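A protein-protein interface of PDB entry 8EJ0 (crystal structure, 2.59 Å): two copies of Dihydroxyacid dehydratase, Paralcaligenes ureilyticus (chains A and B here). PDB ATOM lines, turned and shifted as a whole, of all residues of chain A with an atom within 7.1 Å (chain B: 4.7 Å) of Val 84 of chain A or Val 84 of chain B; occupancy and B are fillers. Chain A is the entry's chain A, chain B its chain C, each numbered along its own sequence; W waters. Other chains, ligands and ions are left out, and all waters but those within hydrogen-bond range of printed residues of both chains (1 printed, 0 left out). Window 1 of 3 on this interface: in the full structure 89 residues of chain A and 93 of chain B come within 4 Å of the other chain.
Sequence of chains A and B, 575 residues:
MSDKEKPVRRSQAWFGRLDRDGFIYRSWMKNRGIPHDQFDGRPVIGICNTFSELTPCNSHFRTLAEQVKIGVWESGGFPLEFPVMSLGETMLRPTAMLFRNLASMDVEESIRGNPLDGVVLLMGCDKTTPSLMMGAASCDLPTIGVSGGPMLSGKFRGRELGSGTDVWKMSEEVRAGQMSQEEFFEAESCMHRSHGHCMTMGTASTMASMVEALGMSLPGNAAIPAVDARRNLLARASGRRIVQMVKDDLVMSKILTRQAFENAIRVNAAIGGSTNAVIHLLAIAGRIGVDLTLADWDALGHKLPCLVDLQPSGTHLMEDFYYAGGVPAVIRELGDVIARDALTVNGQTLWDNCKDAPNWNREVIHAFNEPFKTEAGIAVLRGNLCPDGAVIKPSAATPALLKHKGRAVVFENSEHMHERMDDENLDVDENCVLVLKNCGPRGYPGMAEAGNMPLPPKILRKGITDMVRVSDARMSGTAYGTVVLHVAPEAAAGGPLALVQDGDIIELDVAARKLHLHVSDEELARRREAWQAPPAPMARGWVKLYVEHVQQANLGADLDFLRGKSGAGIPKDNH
The backbone carbonyl oxygen (O) of Phe 82 of chain B lies within hydrogen-bond range of the backbone NH (N) of Asn 49 of chain B (3.0 Å). The side-chain carboxylate of Asp 106 of chain A lies close to the backbone NH of Met 85 of chain A (3.3 Å). The backbone NH (N) of Met 85 of chain B lies within hydrogen-bond range of the side-chain carboxylate (OD2) of Asp 106 of chain B, at 3.1 Å. The backbone NH (N) of Phe 51 of chain A lies within hydrogen-bond range of the side-chain amide oxygen (OD1) of Asn 49 of chain A, at 2.8 Å. The side-chain hydroxyl (OG) of Ser 110 of chain B sits at hydrogen-bond distance from the backbone carbonyl oxygen (O) of Asp 106 of chain B. O of Asp 106 of chain A lies within hydrogen-bond range of OG of Ser 110 of chain A.
The side-chain carboxylate (OD2) of Asp 106 of chain A sits close to the side-chain carboxylate (OD2) of Asp 106 of chain B (2.4 Å).
Of the 12 printed residues of chain B, 7 touch a printed residue of chain A. Hydrophobic or aromatic side chains of chain B within 4 Å of the printed part of chain A: Phe 82, Pro 83 and Met 85. Hydrophobic or aromatic side chains of chain A within 4 Å of the printed part of chain B: Pro 83 and Met 85. Among the printed residues, no Asp or Glu carboxylate lies within 4 Å of a Lys or Arg side-chain nitrogen of the other chain.
Of the printed residues of chain A, Pro 83 of chain B touches Phe 51 (3.1 Å), Ser 52 (3.6 Å), Pro 83 (3.7 Å), Val 84 (3.2 Å) and Met 85 (3.9 Å). Of the printed residues of chain A, Met 85 of chain B touches Pro 83 and Ser 110. Of the printed residues of chain A, Ser 110 of chain B touches Met 85 (3.4 Å). The nearest printed residue of chain A that does not touch Val 84 of chain B is Met 85 of chain A (4.5 Å).
Pro 83 of chain A touches its own counterpart, Pro 83 of chain B. Pro 83 of chain A touches Ser 86 of chain B, but with the chains exchanged Ser 86 of chain A does not touch Pro 83 of chain B (4.1 Å). Val 84 of chain A touches its own counterpart, Val 84 of chain B. Met 85 of chain A touches Asp 106 of chain B, but with the chains exchanged Asp 106 of chain A does not touch Met 85 of chain B (4.2 Å). Positions printed for both chains: 48, 49, 50, 82, 83, 84, 85, 86, 106, 107, 110 and 132.
Water W1 lies within hydrogen-bond range of the backbone carbonyl oxygen of Pro 83 of chain A (2.4 Å), the backbone NH of Ser 86 of chain B (3.0 Å) and the side-chain hydroxyl of Ser 110 of chain A (3.5 Å).
Among the printed residues, pairs that only touch across the chains: Phe 51 of chain A with Pro 83 of chain B, Ser 52 of chain A with Phe 82 of chain B, Ser 52 of chain A with Pro 83 of chain B, Pro 83 of chain A with Pro 83 of chain B, Pro 83 of chain A with Val 84 of chain B, Pro 83 of chain A with Met 85 of chain B, Pro 83 of chain A with Ser 86 of chain B, Val 84 of chain A with Pro 83 of chain B, Val 84 of chain A with Val 84 of chain B, Met 85 of chain A with Pro 83 of chain B, Met 85 of chain A with Asp 106 of chain B, Met 85 of chain A with Ser 110 of chain B and Ser 110 of chain A with Met 85 of chain B.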
ATOM      1  N   CYS A  48     -20.814   2.663  13.098  1.00  0.00           N
ATOM      2  CA  CYS A  48     -21.999   2.625  13.954  1.00  0.00           C
ATOM      3  C   CYS A  48     -22.446   1.176  14.090  1.00  0.00           C
ATOM      4  O   CYS A  48     -23.104   0.627  13.203  1.00  0.00           O
ATOM      5  CB  CYS A  48     -23.109   3.496  13.382  1.00  0.00           C
ATOM      6  SG  CYS A  48     -24.546   3.652  14.464  1.00  0.00           S
ATOM      7  N   ASN A  49     -22.092   0.552  15.210  1.00  0.00           N
ATOM      8  CA  ASN A  49     -22.350  -0.863  15.439  1.00  0.00           C
ATOM      9  C   ASN A  49     -23.651  -1.012  16.218  1.00  0.00           C
ATOM     10  O   ASN A  49     -23.730  -0.628  17.389  1.00  0.00           O
ATOM     11  CB  ASN A  49     -21.189  -1.509  16.190  1.00  0.00           C
ATOM     12  CG  ASN A  49     -21.237  -3.022  16.145  1.00  0.00           C
ATOM     13  OD1 ASN A  49     -22.251  -3.613  15.777  1.00  0.00           O
ATOM     14  ND2 ASN A  49     -20.135  -3.659  16.522  1.00  0.00           N
ATOM     15  N   THR A  50     -24.668  -1.577  15.568  1.00  0.00           N
ATOM     16  CA  THR A  50     -25.924  -1.906  16.223  1.00  0.00           C
ATOM     17  C   THR A  50     -25.951  -3.334  16.748  1.00  0.00           C
ATOM     18  O   THR A  50     -27.038  -3.910  16.889  1.00  0.00           O
ATOM     19  CB  THR A  50     -27.101  -1.683  15.267  1.00  0.00           C
ATOM     20  OG1 THR A  50     -26.921  -2.476  14.088  1.00  0.00           O
ATOM     21  CG2 THR A  50     -27.201  -0.219  14.878  1.00  0.00           C
ATOM     22  N   PHE A  51     -24.787  -3.921  17.027  1.00  0.00           N
ATOM     23  CA  PHE A  51     -24.752  -5.269  17.577  1.00  0.00           C
ATOM     24  C   PHE A  51     -25.521  -5.327  18.887  1.00  0.00           C
ATOM     25  O   PHE A  51     -25.421  -4.428  19.726  1.00  0.00           O
ATOM     26  CB  PHE A  51     -23.317  -5.737  17.819  1.00  0.00           C
ATOM     27  CG  PHE A  51     -23.220  -6.855  18.820  1.00  0.00           C
ATOM     28  CD1 PHE A  51     -23.567  -8.149  18.465  1.00  0.00           C
ATOM     29  CD2 PHE A  51     -22.812  -6.607  20.123  1.00  0.00           C
ATOM     30  CE1 PHE A  51     -23.499  -9.178  19.383  1.00  0.00           C
ATOM     31  CE2 PHE A  51     -22.739  -7.632  21.047  1.00  0.00           C
ATOM     32  CZ  PHE A  51     -23.082  -8.921  20.678  1.00  0.00           C
ATOM     33  N   SER A  52     -26.281  -6.402  19.063  1.00  0.00           N
ATOM     34  CA  SER A  52     -27.026  -6.615  20.292  1.00  0.00           C
ATOM     35  C   SER A  52     -27.431  -8.076  20.367  1.00  0.00           C
ATOM     36  O   SER A  52     -27.778  -8.681  19.350  1.00  0.00           O
ATOM     37  CB  SER A  52     -28.267  -5.719  20.360  1.00  0.00           C
ATOM     38  OG  SER A  52     -29.057  -6.028  21.493  1.00  0.00           O
ATOM     39  N   PHE A  82     -18.597   2.629  17.450  1.00  0.00           N
ATOM     40  CA  PHE A  82     -19.354   3.187  18.558  1.00  0.00           C
ATOM     41  C   PHE A  82     -20.745   2.576  18.577  1.00  0.00           C
ATOM     42  O   PHE A  82     -21.270   2.183  17.527  1.00  0.00           O
ATOM     43  CB  PHE A  82     -19.460   4.719  18.463  1.00  0.00           C
ATOM     44  CG  PHE A  82     -20.128   5.209  17.209  1.00  0.00           C
ATOM     45  CD1 PHE A  82     -19.399   5.406  16.047  1.00  0.00           C
ATOM     46  CD2 PHE A  82     -21.485   5.490  17.196  1.00  0.00           C
ATOM     47  CE1 PHE A  82     -20.012   5.862  14.895  1.00  0.00           C
ATOM     48  CE2 PHE A  82     -22.104   5.946  16.048  1.00  0.00           C
ATOM     49  CZ  PHE A  82     -21.366   6.133  14.896  1.00  0.00           C
ATOM     50  N   PRO A  83     -21.362   2.476  19.751  1.00  0.00           N
ATOM     51  CA  PRO A  83     -22.691   1.863  19.834  1.00  0.00           C
ATOM     52  C   PRO A  83     -23.818   2.881  19.851  1.00  0.00           C
ATOM     53  O   PRO A  83     -23.619   4.047  20.208  1.00  0.00           O
ATOM     54  CB  PRO A  83     -22.622   1.099  21.159  1.00  0.00           C
ATOM     55  CG  PRO A  83     -21.782   2.002  22.017  1.00  0.00           C
ATOM     56  CD  PRO A  83     -20.782   2.683  21.090  1.00  0.00           C
ATOM     57  N   VAL A  84     -25.010   2.442  19.458  1.00  0.00           N
ATOM     58  CA  VAL A  84     -26.246   3.179  19.640  1.00  0.00           C
ATOM     59  C   VAL A  84     -27.281   2.218  20.214  1.00  0.00           C
ATOM     60  O   VAL A  84     -26.986   1.058  20.493  1.00  0.00           O
ATOM     61  CB  VAL A  84     -26.751   3.818  18.331  1.00  0.00           C
ATOM     62  CG1 VAL A  84     -25.775   4.877  17.837  1.00  0.00           C
ATOM     63  CG2 VAL A  84     -26.972   2.748  17.271  1.00  0.00           C
ATOM     64  N   MET A  85     -28.501   2.711  20.393  1.00  0.00           N
ATOM     65  CA  MET A  85     -29.590   1.833  20.791  1.00  0.00           C
ATOM     66  C   MET A  85     -29.956   0.918  19.629  1.00  0.00           C
ATOM     67  O   MET A  85     -30.208   1.385  18.515  1.00  0.00           O
ATOM     68  CB  MET A  85     -30.806   2.644  21.235  1.00  0.00           C
ATOM     69  CG  MET A  85     -31.978   1.791  21.700  1.00  0.00           C
ATOM     70  SD  MET A  85     -33.423   2.763  22.163  1.00  0.00           S
ATOM     71  CE  MET A  85     -34.551   1.474  22.686  1.00  0.00           C
ATOM     72  N   SER A  86     -29.964  -0.385  19.885  1.00  0.00           N
ATOM     73  CA  SER A  86     -30.348  -1.366  18.883  1.00  0.00           C
ATOM     74  C   SER A  86     -31.831  -1.689  19.023  1.00  0.00           C
ATOM     75  O   SER A  86     -32.414  -1.573  20.103  1.00  0.00           O
ATOM     76  CB  SER A  86     -29.511  -2.640  19.014  1.00  0.00           C
ATOM     77  OG  SER A  86     -29.612  -3.438  17.846  1.00  0.00           O
ATOM     78  N   LEU A  87     -32.442  -2.090  17.910  1.00  0.00           N
ATOM     79  CA  LEU A  87     -33.892  -2.257  17.830  1.00  0.00           C
ATOM     80  C   LEU A  87     -34.209  -3.634  17.256  1.00  0.00           C
ATOM     81  O   LEU A  87     -34.186  -3.823  16.037  1.00  0.00           O
ATOM     82  CB  LEU A  87     -34.518  -1.155  16.982  1.00  0.00           C
ATOM     83  CG  LEU A  87     -34.084   0.279  17.298  1.00  0.00           C
ATOM     84  CD1 LEU A  87     -34.640   1.249  16.267  1.00  0.00           C
ATOM     85  CD2 LEU A  87     -34.510   0.682  18.701  1.00  0.00           C
ATOM     86  N   ALA A 103     -33.222   6.101  18.762  1.00  0.00           N
ATOM     87  CA  ALA A 103     -31.900   5.682  18.315  1.00  0.00           C
ATOM     88  C   ALA A 103     -31.384   6.565  17.184  1.00  0.00           C
ATOM     89  O   ALA A 103     -30.168   6.673  16.993  1.00  0.00           O
ATOM     90  CB  ALA A 103     -31.931   4.216  17.887  1.00  0.00           C
ATOM     91  N   SER A 104     -32.285   7.205  16.431  1.00  0.00           N
ATOM     92  CA  SER A 104     -31.844   8.156  15.415  1.00  0.00           C
ATOM     93  C   SER A 104     -31.135   9.346  16.047  1.00  0.00           C
ATOM     94  O   SER A 104     -30.201   9.897  15.455  1.00  0.00           O
ATOM     95  CB  SER A 104     -33.030   8.631  14.576  1.00  0.00           C
ATOM     96  OG  SER A 104     -33.817   9.573  15.283  1.00  0.00           O
ATOM     97  N   MET A 105     -31.567   9.758  17.241  1.00  0.00           N
ATOM     98  CA  MET A 105     -30.846  10.801  17.961  1.00  0.00           C
ATOM     99  C   MET A 105     -29.493  10.299  18.448  1.00  0.00           C
ATOM    100  O   MET A 105     -28.509  11.048  18.439  1.00  0.00           O
ATOM    101  CB  MET A 105     -31.682  11.315  19.133  1.00  0.00           C
ATOM    102  CG  MET A 105     -32.864  12.171  18.719  1.00  0.00           C
ATOM    103  SD  MET A 105     -33.586  13.084  20.096  1.00  0.00           S
ATOM    104  CE  MET A 105     -34.286  11.754  21.069  1.00  0.00           C
ATOM    105  N   ASP A 106     -29.425   9.037  18.883  1.00  0.00           N
ATOM    106  CA  ASP A 106     -28.141   8.444  19.245  1.00  0.00           C
ATOM    107  C   ASP A 106     -27.165   8.519  18.080  1.00  0.00           C
ATOM    108  O   ASP A 106     -26.011   8.932  18.244  1.00  0.00           O
ATOM    109  CB  ASP A 106     -28.330   6.990  19.680  1.00  0.00           C
ATOM    110  CG  ASP A 106     -29.274   6.846  20.853  1.00  0.00           C
ATOM    111  OD1 ASP A 106     -29.490   7.842  21.575  1.00  0.00           O
ATOM    112  OD2 ASP A 106     -29.793   5.728  21.058  1.00  0.00           O
ATOM    113  N   VAL A 107     -27.620   8.128  16.888  1.00  0.00           N
ATOM    114  CA  VAL A 107     -26.763   8.153  15.707  1.00  0.00           C
ATOM    115  C   VAL A 107     -26.306   9.576  15.412  1.00  0.00           C
ATOM    116  O   VAL A 107     -25.107   9.844  15.265  1.00  0.00           O
ATOM    117  CB  VAL A 107     -27.495   7.540  14.500  1.00  0.00           C
ATOM    118  CG1 VAL A 107     -26.655   7.679  13.241  1.00  0.00           C
ATOM    119  CG2 VAL A 107     -27.830   6.083  14.770  1.00  0.00           C
ATOM    120  N   GLU A 108     -27.257  10.509  15.333  1.00  0.00           N
ATOM    121  CA  GLU A 108     -26.937  11.880  14.944  1.00  0.00           C
ATOM    122  C   GLU A 108     -25.939  12.512  15.907  1.00  0.00           C
ATOM    123  O   GLU A 108     -24.932  13.092  15.483  1.00  0.00           O
ATOM    124  CB  GLU A 108     -28.217  12.712  14.878  1.00  0.00           C
ATOM    125  CG  GLU A 108     -28.033  14.072  14.234  1.00  0.00           C
ATOM    126  CD  GLU A 108     -29.194  15.007  14.501  1.00  0.00           C
ATOM    127  OE1 GLU A 108     -28.959  16.232  14.581  1.00  0.00           O
ATOM    128  OE2 GLU A 108     -30.338  14.523  14.636  1.00  0.00           O
ATOM    129  N   SER A 110     -23.949  11.048  18.143  1.00  0.00           N
ATOM    130  CA  SER A 110     -22.667  10.349  18.190  1.00  0.00           C
ATOM    131  C   SER A 110     -21.785  10.720  17.008  1.00  0.00           C
ATOM    132  O   SER A 110     -20.557  10.742  17.135  1.00  0.00           O
ATOM    133  CB  SER A 110     -22.884   8.835  18.228  1.00  0.00           C
ATOM    134  OG  SER A 110     -23.538   8.435  19.420  1.00  0.00           O
ATOM    135  N   LEU A 122     -23.878  -0.015  10.254  1.00  0.00           N
ATOM    136  CA  LEU A 122     -24.149  -1.447  10.347  1.00  0.00           C
ATOM    137  C   LEU A 122     -25.636  -1.612  10.633  1.00  0.00           C
ATOM    138  O   LEU A 122     -26.093  -1.388  11.757  1.00  0.00           O
ATOM    139  CB  LEU A 122     -23.291  -2.101  11.427  1.00  0.00           C
ATOM    140  CG  LEU A 122     -21.777  -2.018  11.234  1.00  0.00           C
ATOM    141  CD1 LEU A 122     -21.061  -2.870  12.271  1.00  0.00           C
ATOM    142  CD2 LEU A 122     -21.387  -2.437   9.824  1.00  0.00           C
ATOM    143  N   SER A 131     -33.232   3.891  11.258  1.00  0.00           N
ATOM    144  CA  SER A 131     -32.723   4.585  12.439  1.00  0.00           C
ATOM    145  C   SER A 131     -31.352   5.191  12.179  1.00  0.00           C
ATOM    146  O   SER A 131     -31.089   6.336  12.564  1.00  0.00           O
ATOM    147  CB  SER A 131     -32.668   3.624  13.623  1.00  0.00           C
ATOM    148  OG  SER A 131     -32.309   4.307  14.806  1.00  0.00           O
ATOM    149  N   LEU A 132     -30.469   4.445  11.515  1.00  0.00           N
ATOM    150  CA  LEU A 132     -29.123   4.945  11.256  1.00  0.00           C
ATOM    151  C   LEU A 132     -29.095   5.885  10.058  1.00  0.00           C
ATOM    152  O   LEU A 132     -28.347   6.868  10.058  1.00  0.00           O
ATOM    153  CB  LEU A 132     -28.158   3.777  11.045  1.00  0.00           C
ATOM    154  CG  LEU A 132     -27.467   3.201  12.286  1.00  0.00           C
ATOM    155  CD1 LEU A 132     -28.475   2.788  13.348  1.00  0.00           C
ATOM    156  CD2 LEU A 132     -26.581   2.026  11.905  1.00  0.00           C
ATOM    157  N   CYS B  48     -26.164  -4.045  30.101  1.00  0.00           N
ATOM    158  CA  CYS B  48     -25.992  -2.773  29.406  1.00  0.00           C
ATOM    159  C   CYS B  48     -24.507  -2.524  29.185  1.00  0.00           C
ATOM    160  O   CYS B  48     -23.774  -2.211  30.128  1.00  0.00           O
ATOM    161  CB  CYS B  48     -26.624  -1.639  30.207  1.00  0.00           C
ATOM    162  SG  CYS B  48     -26.674  -0.060  29.330  1.00  0.00           S
ATOM    163  N   ASN B  49     -24.060  -2.659  27.939  1.00  0.00           N
ATOM    164  CA  ASN B  49     -22.646  -2.564  27.588  1.00  0.00           C
ATOM    165  C   ASN B  49     -22.387  -1.211  26.934  1.00  0.00           C
ATOM    166  O   ASN B  49     -22.883  -0.937  25.837  1.00  0.00           O
ATOM    167  CB  ASN B  49     -22.247  -3.712  26.663  1.00  0.00           C
ATOM    168  CG  ASN B  49     -20.753  -3.773  26.422  1.00  0.00           C
ATOM    169  OD1 ASN B  49     -19.978  -3.068  27.063  1.00  0.00           O
ATOM    170  ND2 ASN B  49     -20.339  -4.633  25.495  1.00  0.00           N
ATOM    171  N   THR B  50     -21.604  -0.369  27.612  1.00  0.00           N
ATOM    172  CA  THR B  50     -21.203   0.929  27.080  1.00  0.00           C
ATOM    173  C   THR B  50     -19.845   0.885  26.393  1.00  0.00           C
ATOM    174  O   THR B  50     -19.152   1.910  26.340  1.00  0.00           O
ATOM    175  CB  THR B  50     -21.194   1.979  28.192  1.00  0.00           C
ATOM    176  OG1 THR B  50     -20.277   1.585  29.221  1.00  0.00           O
ATOM    177  CG2 THR B  50     -22.578   2.133  28.784  1.00  0.00           C
ATOM    178  N   PHE B  82     -26.755  -5.673  25.537  1.00  0.00           N
ATOM    179  CA  PHE B  82     -27.348  -4.720  24.613  1.00  0.00           C
ATOM    180  C   PHE B  82     -26.579  -3.411  24.697  1.00  0.00           C
ATOM    181  O   PHE B  82     -26.005  -3.091  25.744  1.00  0.00           O
ATOM    182  CB  PHE B  82     -28.836  -4.475  24.919  1.00  0.00           C
ATOM    183  CG  PHE B  82     -29.096  -3.945  26.300  1.00  0.00           C
ATOM    184  CD1 PHE B  82     -29.234  -4.810  27.374  1.00  0.00           C
ATOM    185  CD2 PHE B  82     -29.219  -2.583  26.524  1.00  0.00           C
ATOM    186  CE1 PHE B  82     -29.480  -4.327  28.646  1.00  0.00           C
ATOM    187  CE2 PHE B  82     -29.464  -2.094  27.794  1.00  0.00           C
ATOM    188  CZ  PHE B  82     -29.595  -2.968  28.856  1.00  0.00           C
ATOM    189  N   PRO B  83     -26.537  -2.644  23.609  1.00  0.00           N
ATOM    190  CA  PRO B  83     -25.787  -1.385  23.629  1.00  0.00           C
ATOM    191  C   PRO B  83     -26.664  -0.172  23.883  1.00  0.00           C
ATOM    192  O   PRO B  83     -27.873  -0.199  23.646  1.00  0.00           O
ATOM    193  CB  PRO B  83     -25.182  -1.339  22.225  1.00  0.00           C
ATOM    194  CG  PRO B  83     -26.267  -1.940  21.381  1.00  0.00           C
ATOM    195  CD  PRO B  83     -26.949  -3.001  22.239  1.00  0.00           C
ATOM    196  N   VAL B  84     -26.048   0.899  24.376  1.00  0.00           N
ATOM    197  CA  VAL B  84     -26.650   2.218  24.445  1.00  0.00           C
ATOM    198  C   VAL B  84     -25.632   3.217  23.909  1.00  0.00           C
ATOM    199  O   VAL B  84     -24.506   2.856  23.572  1.00  0.00           O
ATOM    200  CB  VAL B  84     -27.099   2.589  25.874  1.00  0.00           C
ATOM    201  CG1 VAL B  84     -28.160   1.622  26.374  1.00  0.00           C
ATOM    202  CG2 VAL B  84     -25.903   2.620  26.815  1.00  0.00           C
ATOM    203  N   MET B  85     -26.040   4.478  23.823  1.00  0.00           N
ATOM    204  CA  MET B  85     -25.100   5.521  23.443  1.00  0.00           C
ATOM    205  C   MET B  85     -24.018   5.646  24.507  1.00  0.00           C
ATOM    206  O   MET B  85     -24.314   5.832  25.690  1.00  0.00           O
ATOM    207  CB  MET B  85     -25.814   6.858  23.257  1.00  0.00           C
ATOM    208  CG  MET B  85     -24.883   7.992  22.847  1.00  0.00           C
ATOM    209  SD  MET B  85     -25.705   9.589  22.704  1.00  0.00           S
ATOM    210  CE  MET B  85     -24.326  10.633  22.244  1.00  0.00           C
ATOM    211  N   SER B  86     -22.762   5.526  24.087  1.00  0.00           N
ATOM    212  CA  SER B  86     -21.642   5.648  25.005  1.00  0.00           C
ATOM    213  C   SER B  86     -21.147   7.088  25.021  1.00  0.00           C
ATOM    214  O   SER B  86     -21.293   7.827  24.044  1.00  0.00           O
ATOM    215  CB  SER B  86     -20.506   4.702  24.615  1.00  0.00           C
ATOM    216  OG  SER B  86     -19.595   4.541  25.690  1.00  0.00           O
ATOM    217  N   ASP B 106     -31.910   5.875  26.237  1.00  0.00           N
ATOM    218  CA  ASP B 106     -31.483   4.601  25.668  1.00  0.00           C
ATOM    219  C   ASP B 106     -31.598   3.492  26.701  1.00  0.00           C
ATOM    220  O   ASP B 106     -32.141   2.418  26.425  1.00  0.00           O
ATOM    221  CB  ASP B 106     -30.042   4.693  25.158  1.00  0.00           C
ATOM    222  CG  ASP B 106     -29.899   5.590  23.948  1.00  0.00           C
ATOM    223  OD1 ASP B 106     -30.816   6.397  23.688  1.00  0.00           O
ATOM    224  OD2 ASP B 106     -28.865   5.484  23.256  1.00  0.00           O
ATOM    225  N   VAL B 107     -31.096   3.749  27.910  1.00  0.00           N
ATOM    226  CA  VAL B 107     -31.067   2.723  28.947  1.00  0.00           C
ATOM    227  C   VAL B 107     -32.480   2.377  29.401  1.00  0.00           C
ATOM    228  O   VAL B 107     -32.863   1.201  29.442  1.00  0.00           O
ATOM    229  CB  VAL B 107     -30.194   3.185  30.127  1.00  0.00           C
ATOM    230  CG1 VAL B 107     -30.217   2.155  31.241  1.00  0.00           C
ATOM    231  CG2 VAL B 107     -28.771   3.444  29.660  1.00  0.00           C
ATOM    232  N   SER B 110     -34.564   0.626  26.569  1.00  0.00           N
ATOM    233  CA  SER B 110     -34.036  -0.697  26.250  1.00  0.00           C
ATOM    234  C   SER B 110     -34.317  -1.695  27.365  1.00  0.00           C
ATOM    235  O   SER B 110     -34.416  -2.900  27.109  1.00  0.00           O
ATOM    236  CB  SER B 110     -32.533  -0.625  25.975  1.00  0.00           C
ATOM    237  OG  SER B 110     -32.263   0.064  24.767  1.00  0.00           O
ATOM    238  N   LEU B 132     -26.561   5.514  32.877  1.00  0.00           N
ATOM    239  CA  LEU B 132     -27.063   4.164  33.112  1.00  0.00           C
ATOM    240  C   LEU B 132     -27.826   4.081  34.427  1.00  0.00           C
ATOM    241  O   LEU B 132     -28.883   3.443  34.499  1.00  0.00           O
ATOM    242  CB  LEU B 132     -25.910   3.162  33.092  1.00  0.00           C
ATOM    243  CG  LEU B 132     -25.625   2.486  31.749  1.00  0.00           C
ATOM    244  CD1 LEU B 132     -25.246   3.512  30.693  1.00  0.00           C
ATOM    245  CD2 LEU B 132     -24.541   1.427  31.896  1.00  0.00           C
HETATM  246  O   HOH W   1     -22.237   5.760  21.183  1.00  0.00           O
